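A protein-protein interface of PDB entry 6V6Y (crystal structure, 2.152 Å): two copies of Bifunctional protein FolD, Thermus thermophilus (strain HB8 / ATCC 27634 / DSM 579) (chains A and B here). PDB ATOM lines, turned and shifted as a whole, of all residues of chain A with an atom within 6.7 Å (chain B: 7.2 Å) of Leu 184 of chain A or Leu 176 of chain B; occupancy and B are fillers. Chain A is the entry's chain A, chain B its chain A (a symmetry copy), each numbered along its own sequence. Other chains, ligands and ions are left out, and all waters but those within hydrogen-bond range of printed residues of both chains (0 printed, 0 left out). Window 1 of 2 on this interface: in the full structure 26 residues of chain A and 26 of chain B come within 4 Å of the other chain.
A ring nitrogen (NE2) of His 186 of chain A lies within hydrogen-bond range of the backbone carbonyl oxygen (O) of Ala 180 of chain B, at 2.7 Å.
O of Leu 176 of chain B is in hydrogen-bond range of NH1 of Arg 163 of chain A (2.7 Å).
The guanidinium group (NH1) of Arg 163 of chain A is in salt-bridge range of the side-chain carboxylate (OD1) of Asp 179 of chain B, at 2.9 Å.
The side-chain amino group (NZ) of Lys 169 of chain A sits at hydrogen-bond distance from the backbone carbonyl oxygen (O) of Trp 128 of chain B (2.9 Å).
The backbone NH of Leu 184 of chain A lies within hydrogen-bond range of the backbone carbonyl oxygen of Val 182 of chain B.
OG1 of Thr 189 of chain A is in hydrogen-bond range of OG1 of Thr 181 of chain B (2.9 Å).
The backbone carbonyl oxygen of Val 182 of chain A lies within hydrogen-bond range of the backbone NH of Leu 184 of chain B (2.9 Å).
The side-chain hydroxyl (OG1) of Thr 183 of chain A lies within hydrogen-bond range of the side-chain hydroxyl (OG1) of Thr 183 of chain B, at 3.0 Å.
The backbone carbonyl oxygen (O) of Thr 183 of chain A is in hydrogen-bond range of the backbone NH (N) of Val 160 of chain A (2.8 Å).
The side-chain hydroxyl (OG1) of Thr 189 of chain A is in hydrogen-bond range of the backbone NH (N) of His 186 of chain A, at 3.0 Å.
O of Val 158 of chain A is in hydrogen-bond range of N of Thr 183 of chain A, at 2.9 Å.
The backbone NH of Ala 180 of chain B is in hydrogen-bond range of the backbone carbonyl oxygen of Leu 175 of chain B, 3.2 Å away.
The backbone carbonyl oxygen (O) of Ser 164 of chain A sits at hydrogen-bond distance from the backbone NH (N) of Lys 169 of chain A.
Among the printed residues, pairs that only touch across the chains: Trp 128 of chain A with Trp 128 of chain B (3.4 Å), Val 182 of chain A with Val 182 of chain B (3.7 Å), Val 182 of chain A with Thr 183 of chain B (3.2 Å), Thr 183 of chain A with Thr 181 of chain B (3.96 Å), Thr 183 of chain A with Val 182 of chain B (3.2 Å), Leu 184 of chain A with Leu 176 of chain B (3.5 Å), Leu 184 of chain A with Thr 181 of chain B (3.7 Å), His 186 of chain A with Leu 176 of chain B (3.96 Å) and His 186 of chain A with Asp 179 of chain B (3.4 Å).
Of the printed residues of chain B, Trp 128 of chain A touches Trp 128 (3.4 Å).
Of the printed residues of chain B, Lys 169 of chain A touches Trp 128 (2.9 Å).
Leu 171 of chain A touches none of the printed residues of chain B.
Leu 184 of chain A touches just these residues of chain B: Leu 176, Thr 181 and Val 182.
Of the printed residues of chain B, Thr 189 of chain A touches Thr 181.
Of chain A, only Arg 163 (2.7 Å), Leu 184 (3.5 Å) and His 186 (3.96 Å) come within 4 Å of Leu 176 of chain B.
Of the printed residues of chain A, Thr 181 of chain B touches Thr 183 (3.96 Å), Leu 184 (3.7 Å) and Thr 189 (2.9 Å).
The nearest residue of chain B that does not touch Leu 184 of chain A is Trp 128 of chain B (4.4 Å).
The nearest residue of chain A that does not touch Leu 176 of chain B is Lys 169 of chain A (4.4 Å).
The nearest printed residue of chain A that does not touch Trp 128 of chain B is Leu 184 of chain A (4.4 Å).
Printed residues of chain A that touch a printed residue of chain B: Trp 128, Arg 163, Lys 169, Val 182, Thr 183, Leu 184, His 186 and Thr 189.
Printed residues of chain B that touch a printed residue of chain A: Trp 128, Leu 176, Asp 179, Ala 180, Thr 181, Val 182, Thr 183 and Leu 184.
Hydrophobic or aromatic side chains of chain B within 4 Å of the printed part of chain A: Trp 128 and Leu 176.
Trp 128 of chain A touches its own counterpart, Trp 128 of chain B.
Val 182 of chain A touches Thr 183 of chain B, and with the chains exchanged Thr 183 of chain A touches Val 182 of chain B.
Val 182 of chain A touches Leu 184 of chain B, and with the chains exchanged Leu 184 of chain A touches Val 182 of chain B.
Thr 183 of chain B touches its own counterpart, Thr 183 of chain A.
Of the 17 pairs that touch across the chains among the printed residues, 7 have their exchanged pair printed and touching as well.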
ATOM      1  N   TRP A 128      -0.277  -0.258  35.053  1.00  0.00           N
ATOM      2  CA  TRP A 128      -0.696  -1.577  34.609  1.00  0.00           C
ATOM      3  C   TRP A 128       0.350  -2.653  34.875  1.00  0.00           C
ATOM      4  O   TRP A 128      -0.013  -3.826  34.959  1.00  0.00           O
ATOM      5  CB  TRP A 128      -1.065  -1.526  33.126  1.00  0.00           C
ATOM      6  CG  TRP A 128      -2.498  -1.013  32.957  1.00  0.00           C
ATOM      7  CD1 TRP A 128      -2.881   0.242  32.592  1.00  0.00           C
ATOM      8  CD2 TRP A 128      -3.713  -1.749  33.194  1.00  0.00           C
ATOM      9  NE1 TRP A 128      -4.256   0.329  32.554  1.00  0.00           N
ATOM     10  CE2 TRP A 128      -4.791  -0.872  32.931  1.00  0.00           C
ATOM     11  CE3 TRP A 128      -3.990  -3.067  33.585  1.00  0.00           C
ATOM     12  CZ2 TRP A 128      -6.130  -1.269  33.048  1.00  0.00           C
ATOM     13  CZ3 TRP A 128      -5.321  -3.466  33.705  1.00  0.00           C
ATOM     14  CH2 TRP A 128      -6.374  -2.568  33.436  1.00  0.00           C
ATOM     15  N   VAL A 158     -16.995  -5.624  40.181  1.00  0.00           N
ATOM     16  CA  VAL A 158     -17.060  -4.221  39.791  1.00  0.00           C
ATOM     17  C   VAL A 158     -17.287  -4.123  38.289  1.00  0.00           C
ATOM     18  O   VAL A 158     -16.550  -4.736  37.500  1.00  0.00           O
ATOM     19  CB  VAL A 158     -15.781  -3.467  40.189  1.00  0.00           C
ATOM     20  CG1 VAL A 158     -15.897  -2.009  39.800  1.00  0.00           C
ATOM     21  CG2 VAL A 158     -15.517  -3.629  41.677  1.00  0.00           C
ATOM     22  N   VAL A 159     -18.301  -3.348  37.890  1.00  0.00           N
ATOM     23  CA  VAL A 159     -18.481  -2.943  36.498  1.00  0.00           C
ATOM     24  C   VAL A 159     -18.128  -1.465  36.358  1.00  0.00           C
ATOM     25  O   VAL A 159     -18.611  -0.617  37.121  1.00  0.00           O
ATOM     26  CB  VAL A 159     -19.904  -3.227  35.986  1.00  0.00           C
ATOM     27  CG1 VAL A 159     -20.061  -2.711  34.550  1.00  0.00           C
ATOM     28  CG2 VAL A 159     -20.222  -4.724  36.066  1.00  0.00           C
ATOM     29  N   VAL A 160     -17.260  -1.169  35.400  1.00  0.00           N
ATOM     30  CA  VAL A 160     -16.880   0.185  35.036  1.00  0.00           C
ATOM     31  C   VAL A 160     -17.462   0.441  33.651  1.00  0.00           C
ATOM     32  O   VAL A 160     -17.178  -0.313  32.709  1.00  0.00           O
ATOM     33  CB  VAL A 160     -15.350   0.332  35.041  1.00  0.00           C
ATOM     34  CG1 VAL A 160     -14.918   1.721  34.625  1.00  0.00           C
ATOM     35  CG2 VAL A 160     -14.794  -0.077  36.403  1.00  0.00           C
ATOM     36  N   VAL A 161     -18.312   1.457  33.521  1.00  0.00           N
ATOM     37  CA  VAL A 161     -18.906   1.784  32.228  1.00  0.00           C
ATOM     38  C   VAL A 161     -18.234   3.029  31.682  1.00  0.00           C
ATOM     39  O   VAL A 161     -18.376   4.122  32.241  1.00  0.00           O
ATOM     40  CB  VAL A 161     -20.427   1.973  32.307  1.00  0.00           C
ATOM     41  CG1 VAL A 161     -21.002   2.068  30.885  1.00  0.00           C
ATOM     42  CG2 VAL A 161     -21.098   0.821  33.091  1.00  0.00           C
ATOM     43  N   GLY A 162     -17.536   2.864  30.561  1.00  0.00           N
ATOM     44  CA  GLY A 162     -16.737   3.915  29.976  1.00  0.00           C
ATOM     45  C   GLY A 162     -15.293   3.481  30.011  1.00  0.00           C
ATOM     46  O   GLY A 162     -14.836   2.925  31.015  1.00  0.00           O
ATOM     47  N   ARG A 163     -14.557   3.715  28.935  1.00  0.00           N
ATOM     48  CA  ARG A 163     -13.217   3.165  28.821  1.00  0.00           C
ATOM     49  C   ARG A 163     -12.220   4.235  28.395  1.00  0.00           C
ATOM     50  O   ARG A 163     -11.307   3.975  27.603  1.00  0.00           O
ATOM     51  CB  ARG A 163     -13.199   1.989  27.840  1.00  0.00           C
ATOM     52  CG  ARG A 163     -13.700   2.374  26.468  1.00  0.00           C
ATOM     53  CD  ARG A 163     -13.411   1.329  25.405  1.00  0.00           C
ATOM     54  NE  ARG A 163     -14.232   1.614  24.235  1.00  0.00           N
ATOM     55  CZ  ARG A 163     -14.215   0.921  23.103  1.00  0.00           C
ATOM     56  NH1 ARG A 163     -13.400  -0.112  22.964  1.00  0.00           N
ATOM     57  NH2 ARG A 163     -15.020   1.271  22.107  1.00  0.00           N
ATOM     58  N   SER A 164     -12.365   5.456  28.913  1.00  0.00           N
ATOM     59  CA  SER A 164     -11.453   6.523  28.519  1.00  0.00           C
ATOM     60  C   SER A 164     -10.107   6.375  29.223  1.00  0.00           C
ATOM     61  O   SER A 164      -9.966   5.628  30.201  1.00  0.00           O
ATOM     62  CB  SER A 164     -12.052   7.886  28.847  1.00  0.00           C
ATOM     63  OG  SER A 164     -11.858   8.143  30.221  1.00  0.00           O
ATOM     64  N   VAL A 167     -10.550   8.159  32.817  1.00  0.00           N
ATOM     65  CA  VAL A 167     -11.259   7.490  33.915  1.00  0.00           C
ATOM     66  C   VAL A 167     -11.251   5.959  33.793  1.00  0.00           C
ATOM     67  O   VAL A 167     -10.618   5.262  34.601  1.00  0.00           O
ATOM     68  CB  VAL A 167     -12.711   8.004  34.022  1.00  0.00           C
ATOM     69  CG1 VAL A 167     -13.404   7.352  35.191  1.00  0.00           C
ATOM     70  CG2 VAL A 167     -12.749   9.526  34.142  1.00  0.00           C
ATOM     71  N   GLY A 168     -11.979   5.417  32.816  1.00  0.00           N
ATOM     72  CA  GLY A 168     -12.340   3.998  32.869  1.00  0.00           C
ATOM     73  C   GLY A 168     -11.152   3.050  32.911  1.00  0.00           C
ATOM     74  O   GLY A 168     -11.080   2.149  33.760  1.00  0.00           O
ATOM     75  N   LYS A 169     -10.198   3.239  31.998  1.00  0.00           N
ATOM     76  CA  LYS A 169      -9.068   2.312  31.928  1.00  0.00           C
ATOM     77  C   LYS A 169      -8.113   2.421  33.117  1.00  0.00           C
ATOM     78  O   LYS A 169      -7.795   1.379  33.718  1.00  0.00           O
ATOM     79  CB  LYS A 169      -8.349   2.481  30.586  1.00  0.00           C
ATOM     80  CG  LYS A 169      -9.207   2.012  29.421  1.00  0.00           C
ATOM     81  CD  LYS A 169      -8.378   1.891  28.140  1.00  0.00           C
ATOM     82  CE  LYS A 169      -8.101   3.253  27.552  1.00  0.00           C
ATOM     83  NZ  LYS A 169      -7.754   3.148  26.106  1.00  0.00           N
ATOM     84  N   LEU A 171      -8.978   3.426  35.988  1.00  0.00           N
ATOM     85  CA  LEU A 171      -9.814   2.893  37.064  1.00  0.00           C
ATOM     86  C   LEU A 171      -9.766   1.371  37.092  1.00  0.00           C
ATOM     87  O   LEU A 171      -9.534   0.759  38.149  1.00  0.00           O
ATOM     88  CB  LEU A 171     -11.260   3.366  36.929  1.00  0.00           C
ATOM     89  CG  LEU A 171     -12.103   2.898  38.135  1.00  0.00           C
ATOM     90  CD1 LEU A 171     -11.412   3.224  39.479  1.00  0.00           C
ATOM     91  CD2 LEU A 171     -13.480   3.502  38.099  1.00  0.00           C
ATOM     92  N   ALA A 172      -9.979   0.739  35.931  1.00  0.00           N
ATOM     93  CA  ALA A 172      -9.929  -0.721  35.887  1.00  0.00           C
ATOM     94  C   ALA A 172      -8.595  -1.238  36.411  1.00  0.00           C
ATOM     95  O   ALA A 172      -8.559  -2.189  37.204  1.00  0.00           O
ATOM     96  CB  ALA A 172     -10.178  -1.216  34.463  1.00  0.00           C
ATOM     97  N   GLY A 173      -7.490  -0.597  36.011  1.00  0.00           N
ATOM     98  CA  GLY A 173      -6.184  -1.010  36.506  1.00  0.00           C
ATOM     99  C   GLY A 173      -6.044  -0.862  38.010  1.00  0.00           C
ATOM    100  O   GLY A 173      -5.484  -1.737  38.681  1.00  0.00           O
ATOM    101  N   VAL A 182     -13.127  -7.171  37.570  1.00  0.00           N
ATOM    102  CA  VAL A 182     -13.430  -5.937  36.858  1.00  0.00           C
ATOM    103  C   VAL A 182     -13.999  -6.246  35.485  1.00  0.00           C
ATOM    104  O   VAL A 182     -13.433  -7.042  34.733  1.00  0.00           O
ATOM    105  CB  VAL A 182     -12.189  -5.039  36.740  1.00  0.00           C
ATOM    106  CG1 VAL A 182     -12.529  -3.823  35.904  1.00  0.00           C
ATOM    107  CG2 VAL A 182     -11.729  -4.614  38.140  1.00  0.00           C
ATOM    108  N   THR A 183     -15.107  -5.598  35.154  1.00  0.00           N
ATOM    109  CA  THR A 183     -15.689  -5.633  33.820  1.00  0.00           C
ATOM    110  C   THR A 183     -15.609  -4.219  33.276  1.00  0.00           C
ATOM    111  O   THR A 183     -16.089  -3.271  33.927  1.00  0.00           O
ATOM    112  CB  THR A 183     -17.140  -6.133  33.857  1.00  0.00           C
ATOM    113  OG1 THR A 183     -17.166  -7.442  34.418  1.00  0.00           O
ATOM    114  CG2 THR A 183     -17.747  -6.197  32.473  1.00  0.00           C
ATOM    115  N   LEU A 184     -14.974  -4.067  32.113  1.00  0.00           N
ATOM    116  CA  LEU A 184     -14.955  -2.793  31.402  1.00  0.00           C
ATOM    117  C   LEU A 184     -16.024  -2.844  30.314  1.00  0.00           C
ATOM    118  O   LEU A 184     -15.930  -3.644  29.370  1.00  0.00           O
ATOM    119  CB  LEU A 184     -13.578  -2.489  30.815  1.00  0.00           C
ATOM    120  CG  LEU A 184     -12.643  -1.594  31.640  1.00  0.00           C
ATOM    121  CD1 LEU A 184     -11.214  -1.630  31.109  1.00  0.00           C
ATOM    122  CD2 LEU A 184     -13.132  -0.142  31.707  1.00  0.00           C
ATOM    123  N   ALA A 185     -17.046  -2.001  30.456  1.00  0.00           N
ATOM    124  CA  ALA A 185     -18.108  -1.866  29.470  1.00  0.00           C
ATOM    125  C   ALA A 185     -18.018  -0.493  28.818  1.00  0.00           C
ATOM    126  O   ALA A 185     -17.288   0.397  29.277  1.00  0.00           O
ATOM    127  CB  ALA A 185     -19.489  -2.092  30.111  1.00  0.00           C
ATOM    128  N   HIS A 186     -18.746  -0.323  27.725  1.00  0.00           N
ATOM    129  CA  HIS A 186     -18.548   0.860  26.884  1.00  0.00           C
ATOM    130  C   HIS A 186     -19.672   0.901  25.862  1.00  0.00           C
ATOM    131  O   HIS A 186     -20.615   0.097  25.914  1.00  0.00           O
ATOM    132  CB  HIS A 186     -17.180   0.834  26.202  1.00  0.00           C
ATOM    133  CG  HIS A 186     -16.867  -0.487  25.576  1.00  0.00           C
ATOM    134  ND1 HIS A 186     -17.536  -0.962  24.467  1.00  0.00           N
ATOM    135  CD2 HIS A 186     -15.990  -1.458  25.931  1.00  0.00           C
ATOM    136  CE1 HIS A 186     -17.055  -2.150  24.144  1.00  0.00           C
ATOM    137  NE2 HIS A 186     -16.125  -2.479  25.022  1.00  0.00           N
ATOM    138  N   THR A 189     -20.783  -2.391  24.145  1.00  0.00           N
ATOM    139  CA  THR A 189     -21.336  -3.496  24.919  1.00  0.00           C
ATOM    140  C   THR A 189     -22.778  -3.736  24.494  1.00  0.00           C
ATOM    141  O   THR A 189     -23.544  -2.789  24.301  1.00  0.00           O
ATOM    142  CB  THR A 189     -21.267  -3.176  26.414  1.00  0.00           C
ATOM    143  OG1 THR A 189     -19.908  -2.872  26.771  1.00  0.00           O
ATOM    144  CG2 THR A 189     -21.786  -4.340  27.243  1.00  0.00           C
ATOM    145  N   VAL A 195     -25.371  -6.281  31.794  1.00  0.00           N
ATOM    146  CA  VAL A 195     -24.006  -6.267  32.309  1.00  0.00           C
ATOM    147  C   VAL A 195     -23.953  -5.502  33.620  1.00  0.00           C
ATOM    148  O   VAL A 195     -23.384  -5.977  34.612  1.00  0.00           O
ATOM    149  CB  VAL A 195     -23.033  -5.676  31.275  1.00  0.00           C
ATOM    150  CG1 VAL A 195     -21.647  -5.527  31.885  1.00  0.00           C
ATOM    151  CG2 VAL A 195     -22.987  -6.557  30.036  1.00  0.00           C
ATOM    152  N   TRP B 128      -2.225   0.690  26.600  1.00  0.00           N
ATOM    153  CA  TRP B 128      -3.423   1.101  27.314  1.00  0.00           C
ATOM    154  C   TRP B 128      -3.879   2.508  26.950  1.00  0.00           C
ATOM    155  O   TRP B 128      -5.058   2.813  27.124  1.00  0.00           O
ATOM    156  CB  TRP B 128      -3.191   0.972  28.820  1.00  0.00           C
ATOM    157  CG  TRP B 128      -3.419  -0.475  29.268  1.00  0.00           C
ATOM    158  CD1 TRP B 128      -2.465  -1.409  29.537  1.00  0.00           C
ATOM    159  CD2 TRP B 128      -4.685  -1.135  29.447  1.00  0.00           C
ATOM    160  NE1 TRP B 128      -3.054  -2.600  29.903  1.00  0.00           N
ATOM    161  CE2 TRP B 128      -4.413  -2.464  29.844  1.00  0.00           C
ATOM    162  CE3 TRP B 128      -6.021  -0.723  29.324  1.00  0.00           C
ATOM    163  CZ2 TRP B 128      -5.427  -3.390  30.121  1.00  0.00           C
ATOM    164  CZ3 TRP B 128      -7.034  -1.643  29.598  1.00  0.00           C
ATOM    165  CH2 TRP B 128      -6.729  -2.962  29.992  1.00  0.00           C
ATOM    166  N   PRO B 170      -2.197  -7.266  29.361  1.00  0.00           N
ATOM    167  CA  PRO B 170      -2.125  -6.790  27.967  1.00  0.00           C
ATOM    168  C   PRO B 170      -3.223  -7.417  27.093  1.00  0.00           C
ATOM    169  O   PRO B 170      -3.769  -6.735  26.210  1.00  0.00           O
ATOM    170  CB  PRO B 170      -0.710  -7.180  27.517  1.00  0.00           C
ATOM    171  CG  PRO B 170      -0.206  -8.159  28.529  1.00  0.00           C
ATOM    172  CD  PRO B 170      -0.949  -7.919  29.803  1.00  0.00           C
ATOM    173  N   LEU B 171      -3.621  -8.672  27.355  1.00  0.00           N
ATOM    174  CA  LEU B 171      -4.743  -9.239  26.607  1.00  0.00           C
ATOM    175  C   LEU B 171      -5.999  -8.398  26.782  1.00  0.00           C
ATOM    176  O   LEU B 171      -6.662  -8.027  25.797  1.00  0.00           O
ATOM    177  CB  LEU B 171      -5.019 -10.681  27.031  1.00  0.00           C
ATOM    178  CG  LEU B 171      -6.122 -11.307  26.151  1.00  0.00           C
ATOM    179  CD1 LEU B 171      -5.847 -11.090  24.645  1.00  0.00           C
ATOM    180  CD2 LEU B 171      -6.280 -12.774  26.444  1.00  0.00           C
ATOM    181  N   ALA B 172      -6.344  -8.078  28.036  1.00  0.00           N
ATOM    182  CA  ALA B 172      -7.529  -7.257  28.271  1.00  0.00           C
ATOM    183  C   ALA B 172      -7.441  -5.941  27.508  1.00  0.00           C
ATOM    184  O   ALA B 172      -8.417  -5.518  26.873  1.00  0.00           O
ATOM    185  CB  ALA B 172      -7.710  -7.004  29.766  1.00  0.00           C
ATOM    186  N   GLY B 173      -6.268  -5.299  27.526  1.00  0.00           N
ATOM    187  CA  GLY B 173      -6.099  -4.058  26.784  1.00  0.00           C
ATOM    188  C   GLY B 173      -6.282  -4.229  25.287  1.00  0.00           C
ATOM    189  O   GLY B 173      -6.907  -3.392  24.628  1.00  0.00           O
ATOM    190  N   LEU B 174      -5.720  -5.307  24.719  1.00  0.00           N
ATOM    191  CA  LEU B 174      -5.867  -5.523  23.281  1.00  0.00           C
ATOM    192  C   LEU B 174      -7.311  -5.853  22.911  1.00  0.00           C
ATOM    193  O   LEU B 174      -7.810  -5.393  21.876  1.00  0.00           O
ATOM    194  CB  LEU B 174      -4.922  -6.630  22.806  1.00  0.00           C
ATOM    195  CG  LEU B 174      -3.441  -6.270  22.923  1.00  0.00           C
ATOM    196  CD1 LEU B 174      -2.578  -7.416  22.378  1.00  0.00           C
ATOM    197  CD2 LEU B 174      -3.121  -4.953  22.193  1.00  0.00           C
ATOM    198  N   LEU B 175      -8.007  -6.636  23.744  1.00  0.00           N
ATOM    199  CA  LEU B 175      -9.406  -6.943  23.442  1.00  0.00           C
ATOM    200  C   LEU B 175     -10.290  -5.701  23.461  1.00  0.00           C
ATOM    201  O   LEU B 175     -11.245  -5.614  22.682  1.00  0.00           O
ATOM    202  CB  LEU B 175      -9.936  -7.976  24.414  1.00  0.00           C
ATOM    203  CG  LEU B 175      -9.294  -9.347  24.233  1.00  0.00           C
ATOM    204  CD1 LEU B 175      -9.556 -10.205  25.481  1.00  0.00           C
ATOM    205  CD2 LEU B 175      -9.816 -10.012  22.963  1.00  0.00           C
ATOM    206  N   LEU B 176      -9.999  -4.730  24.337  1.00  0.00           N
ATOM    207  CA  LEU B 176     -10.789  -3.500  24.328  1.00  0.00           C
ATOM    208  C   LEU B 176     -10.644  -2.757  23.017  1.00  0.00           C
ATOM    209  O   LEU B 176     -11.594  -2.109  22.556  1.00  0.00           O
ATOM    210  CB  LEU B 176     -10.374  -2.568  25.467  1.00  0.00           C
ATOM    211  CG  LEU B 176     -10.869  -2.942  26.845  1.00  0.00           C
ATOM    212  CD1 LEU B 176     -10.008  -2.175  27.830  1.00  0.00           C
ATOM    213  CD2 LEU B 176     -12.377  -2.661  27.015  1.00  0.00           C
ATOM    214  N   ARG B 177      -9.456  -2.811  22.417  1.00  0.00           N
ATOM    215  CA  ARG B 177      -9.263  -2.179  21.120  1.00  0.00           C
ATOM    216  C   ARG B 177     -10.084  -2.842  20.024  1.00  0.00           C
ATOM    217  O   ARG B 177     -10.343  -2.207  18.999  1.00  0.00           O
ATOM    218  CB  ARG B 177      -7.797  -2.207  20.730  1.00  0.00           C
ATOM    219  CG  ARG B 177      -6.904  -1.352  21.560  1.00  0.00           C
ATOM    220  CD  ARG B 177      -5.569  -1.387  20.879  1.00  0.00           C
ATOM    221  NE  ARG B 177      -4.592  -0.595  21.573  1.00  0.00           N
ATOM    222  CZ  ARG B 177      -3.519  -0.075  20.992  1.00  0.00           C
ATOM    223  NH1 ARG B 177      -3.303  -0.284  19.710  1.00  0.00           N
ATOM    224  NH2 ARG B 177      -2.669   0.659  21.698  1.00  0.00           N
ATOM    225  N   GLU B 178     -10.481  -4.100  20.211  1.00  0.00           N
ATOM    226  CA  GLU B 178     -11.397  -4.782  19.304  1.00  0.00           C
ATOM    227  C   GLU B 178     -12.857  -4.591  19.707  1.00  0.00           C
ATOM    228  O   GLU B 178     -13.738  -5.242  19.125  1.00  0.00           O
ATOM    229  CB  GLU B 178     -11.081  -6.284  19.238  1.00  0.00           C
ATOM    230  CG  GLU B 178      -9.611  -6.637  19.087  1.00  0.00           C
ATOM    231  CD  GLU B 178      -9.019  -6.160  17.761  1.00  0.00           C
ATOM    232  OE1 GLU B 178      -9.791  -5.888  16.821  1.00  0.00           O
ATOM    233  OE2 GLU B 178      -7.777  -6.053  17.665  1.00  0.00           O
ATOM    234  N   ASP B 179     -13.125  -3.734  20.705  1.00  0.00           N
ATOM    235  CA  ASP B 179     -14.480  -3.389  21.132  1.00  0.00           C
ATOM    236  C   ASP B 179     -15.198  -4.551  21.799  1.00  0.00           C
ATOM    237  O   ASP B 179     -16.433  -4.601  21.804  1.00  0.00           O
ATOM    238  CB  ASP B 179     -15.326  -2.841  19.975  1.00  0.00           C
ATOM    239  CG  ASP B 179     -14.868  -1.457  19.522  1.00  0.00           C
ATOM    240  OD1 ASP B 179     -14.133  -0.781  20.283  1.00  0.00           O
ATOM    241  OD2 ASP B 179     -15.246  -1.040  18.407  1.00  0.00           O
ATOM    242  N   ALA B 180     -14.447  -5.476  22.389  1.00  0.00           N
ATOM    243  CA  ALA B 180     -15.040  -6.485  23.260  1.00  0.00           C
ATOM    244  C   ALA B 180     -15.411  -5.883  24.621  1.00  0.00           C
ATOM    245  O   ALA B 180     -14.829  -4.891  25.065  1.00  0.00           O
ATOM    246  CB  ALA B 180     -14.067  -7.647  23.476  1.00  0.00           C
ATOM    247  N   THR B 181     -16.379  -6.520  25.291  1.00  0.00           N
ATOM    248  CA  THR B 181     -16.638  -6.290  26.706  1.00  0.00           C
ATOM    249  C   THR B 181     -15.784  -7.271  27.503  1.00  0.00           C
ATOM    250  O   THR B 181     -15.919  -8.486  27.342  1.00  0.00           O
ATOM    251  CB  THR B 181     -18.119  -6.476  27.044  1.00  0.00           C
ATOM    252  OG1 THR B 181     -18.906  -5.511  26.331  1.00  0.00           O
ATOM    253  CG2 THR B 181     -18.351  -6.318  28.557  1.00  0.00           C
ATOM    254  N   VAL B 182     -14.905  -6.752  28.357  1.00  0.00           N
ATOM    255  CA  VAL B 182     -13.843  -7.560  28.942  1.00  0.00           C
ATOM    256  C   VAL B 182     -14.037  -7.680  30.444  1.00  0.00           C
ATOM    257  O   VAL B 182     -14.239  -6.680  31.135  1.00  0.00           O
ATOM    258  CB  VAL B 182     -12.457  -6.980  28.621  1.00  0.00           C
ATOM    259  CG1 VAL B 182     -11.397  -7.792  29.336  1.00  0.00           C
ATOM    260  CG2 VAL B 182     -12.226  -7.017  27.105  1.00  0.00           C
ATOM    261  N   THR B 183     -13.953  -8.904  30.947  1.00  0.00           N
ATOM    262  CA  THR B 183     -13.934  -9.185  32.375  1.00  0.00           C
ATOM    263  C   THR B 183     -12.576  -9.791  32.678  1.00  0.00           C
ATOM    264  O   THR B 183     -12.180 -10.785  32.040  1.00  0.00           O
ATOM    265  CB  THR B 183     -15.069 -10.139  32.770  1.00  0.00           C
ATOM    266  OG1 THR B 183     -16.317  -9.547  32.423  1.00  0.00           O
ATOM    267  CG2 THR B 183     -15.074 -10.420  34.257  1.00  0.00           C
ATOM    268  N   LEU B 184     -11.849  -9.177  33.613  1.00  0.00           N
ATOM    269  CA  LEU B 184     -10.597  -9.736  34.111  1.00  0.00           C
ATOM    270  C   LEU B 184     -10.890 -10.451  35.427  1.00  0.00           C
ATOM    271  O   LEU B 184     -11.279  -9.817  36.420  1.00  0.00           O
ATOM    272  CB  LEU B 184      -9.525  -8.663  34.288  1.00  0.00           C
ATOM    273  CG  LEU B 184      -8.526  -8.470  33.138  1.00  0.00           C
ATOM    274  CD1 LEU B 184      -7.726  -7.181  33.297  1.00  0.00           C
ATOM    275  CD2 LEU B 184      -7.566  -9.657  32.993  1.00  0.00           C
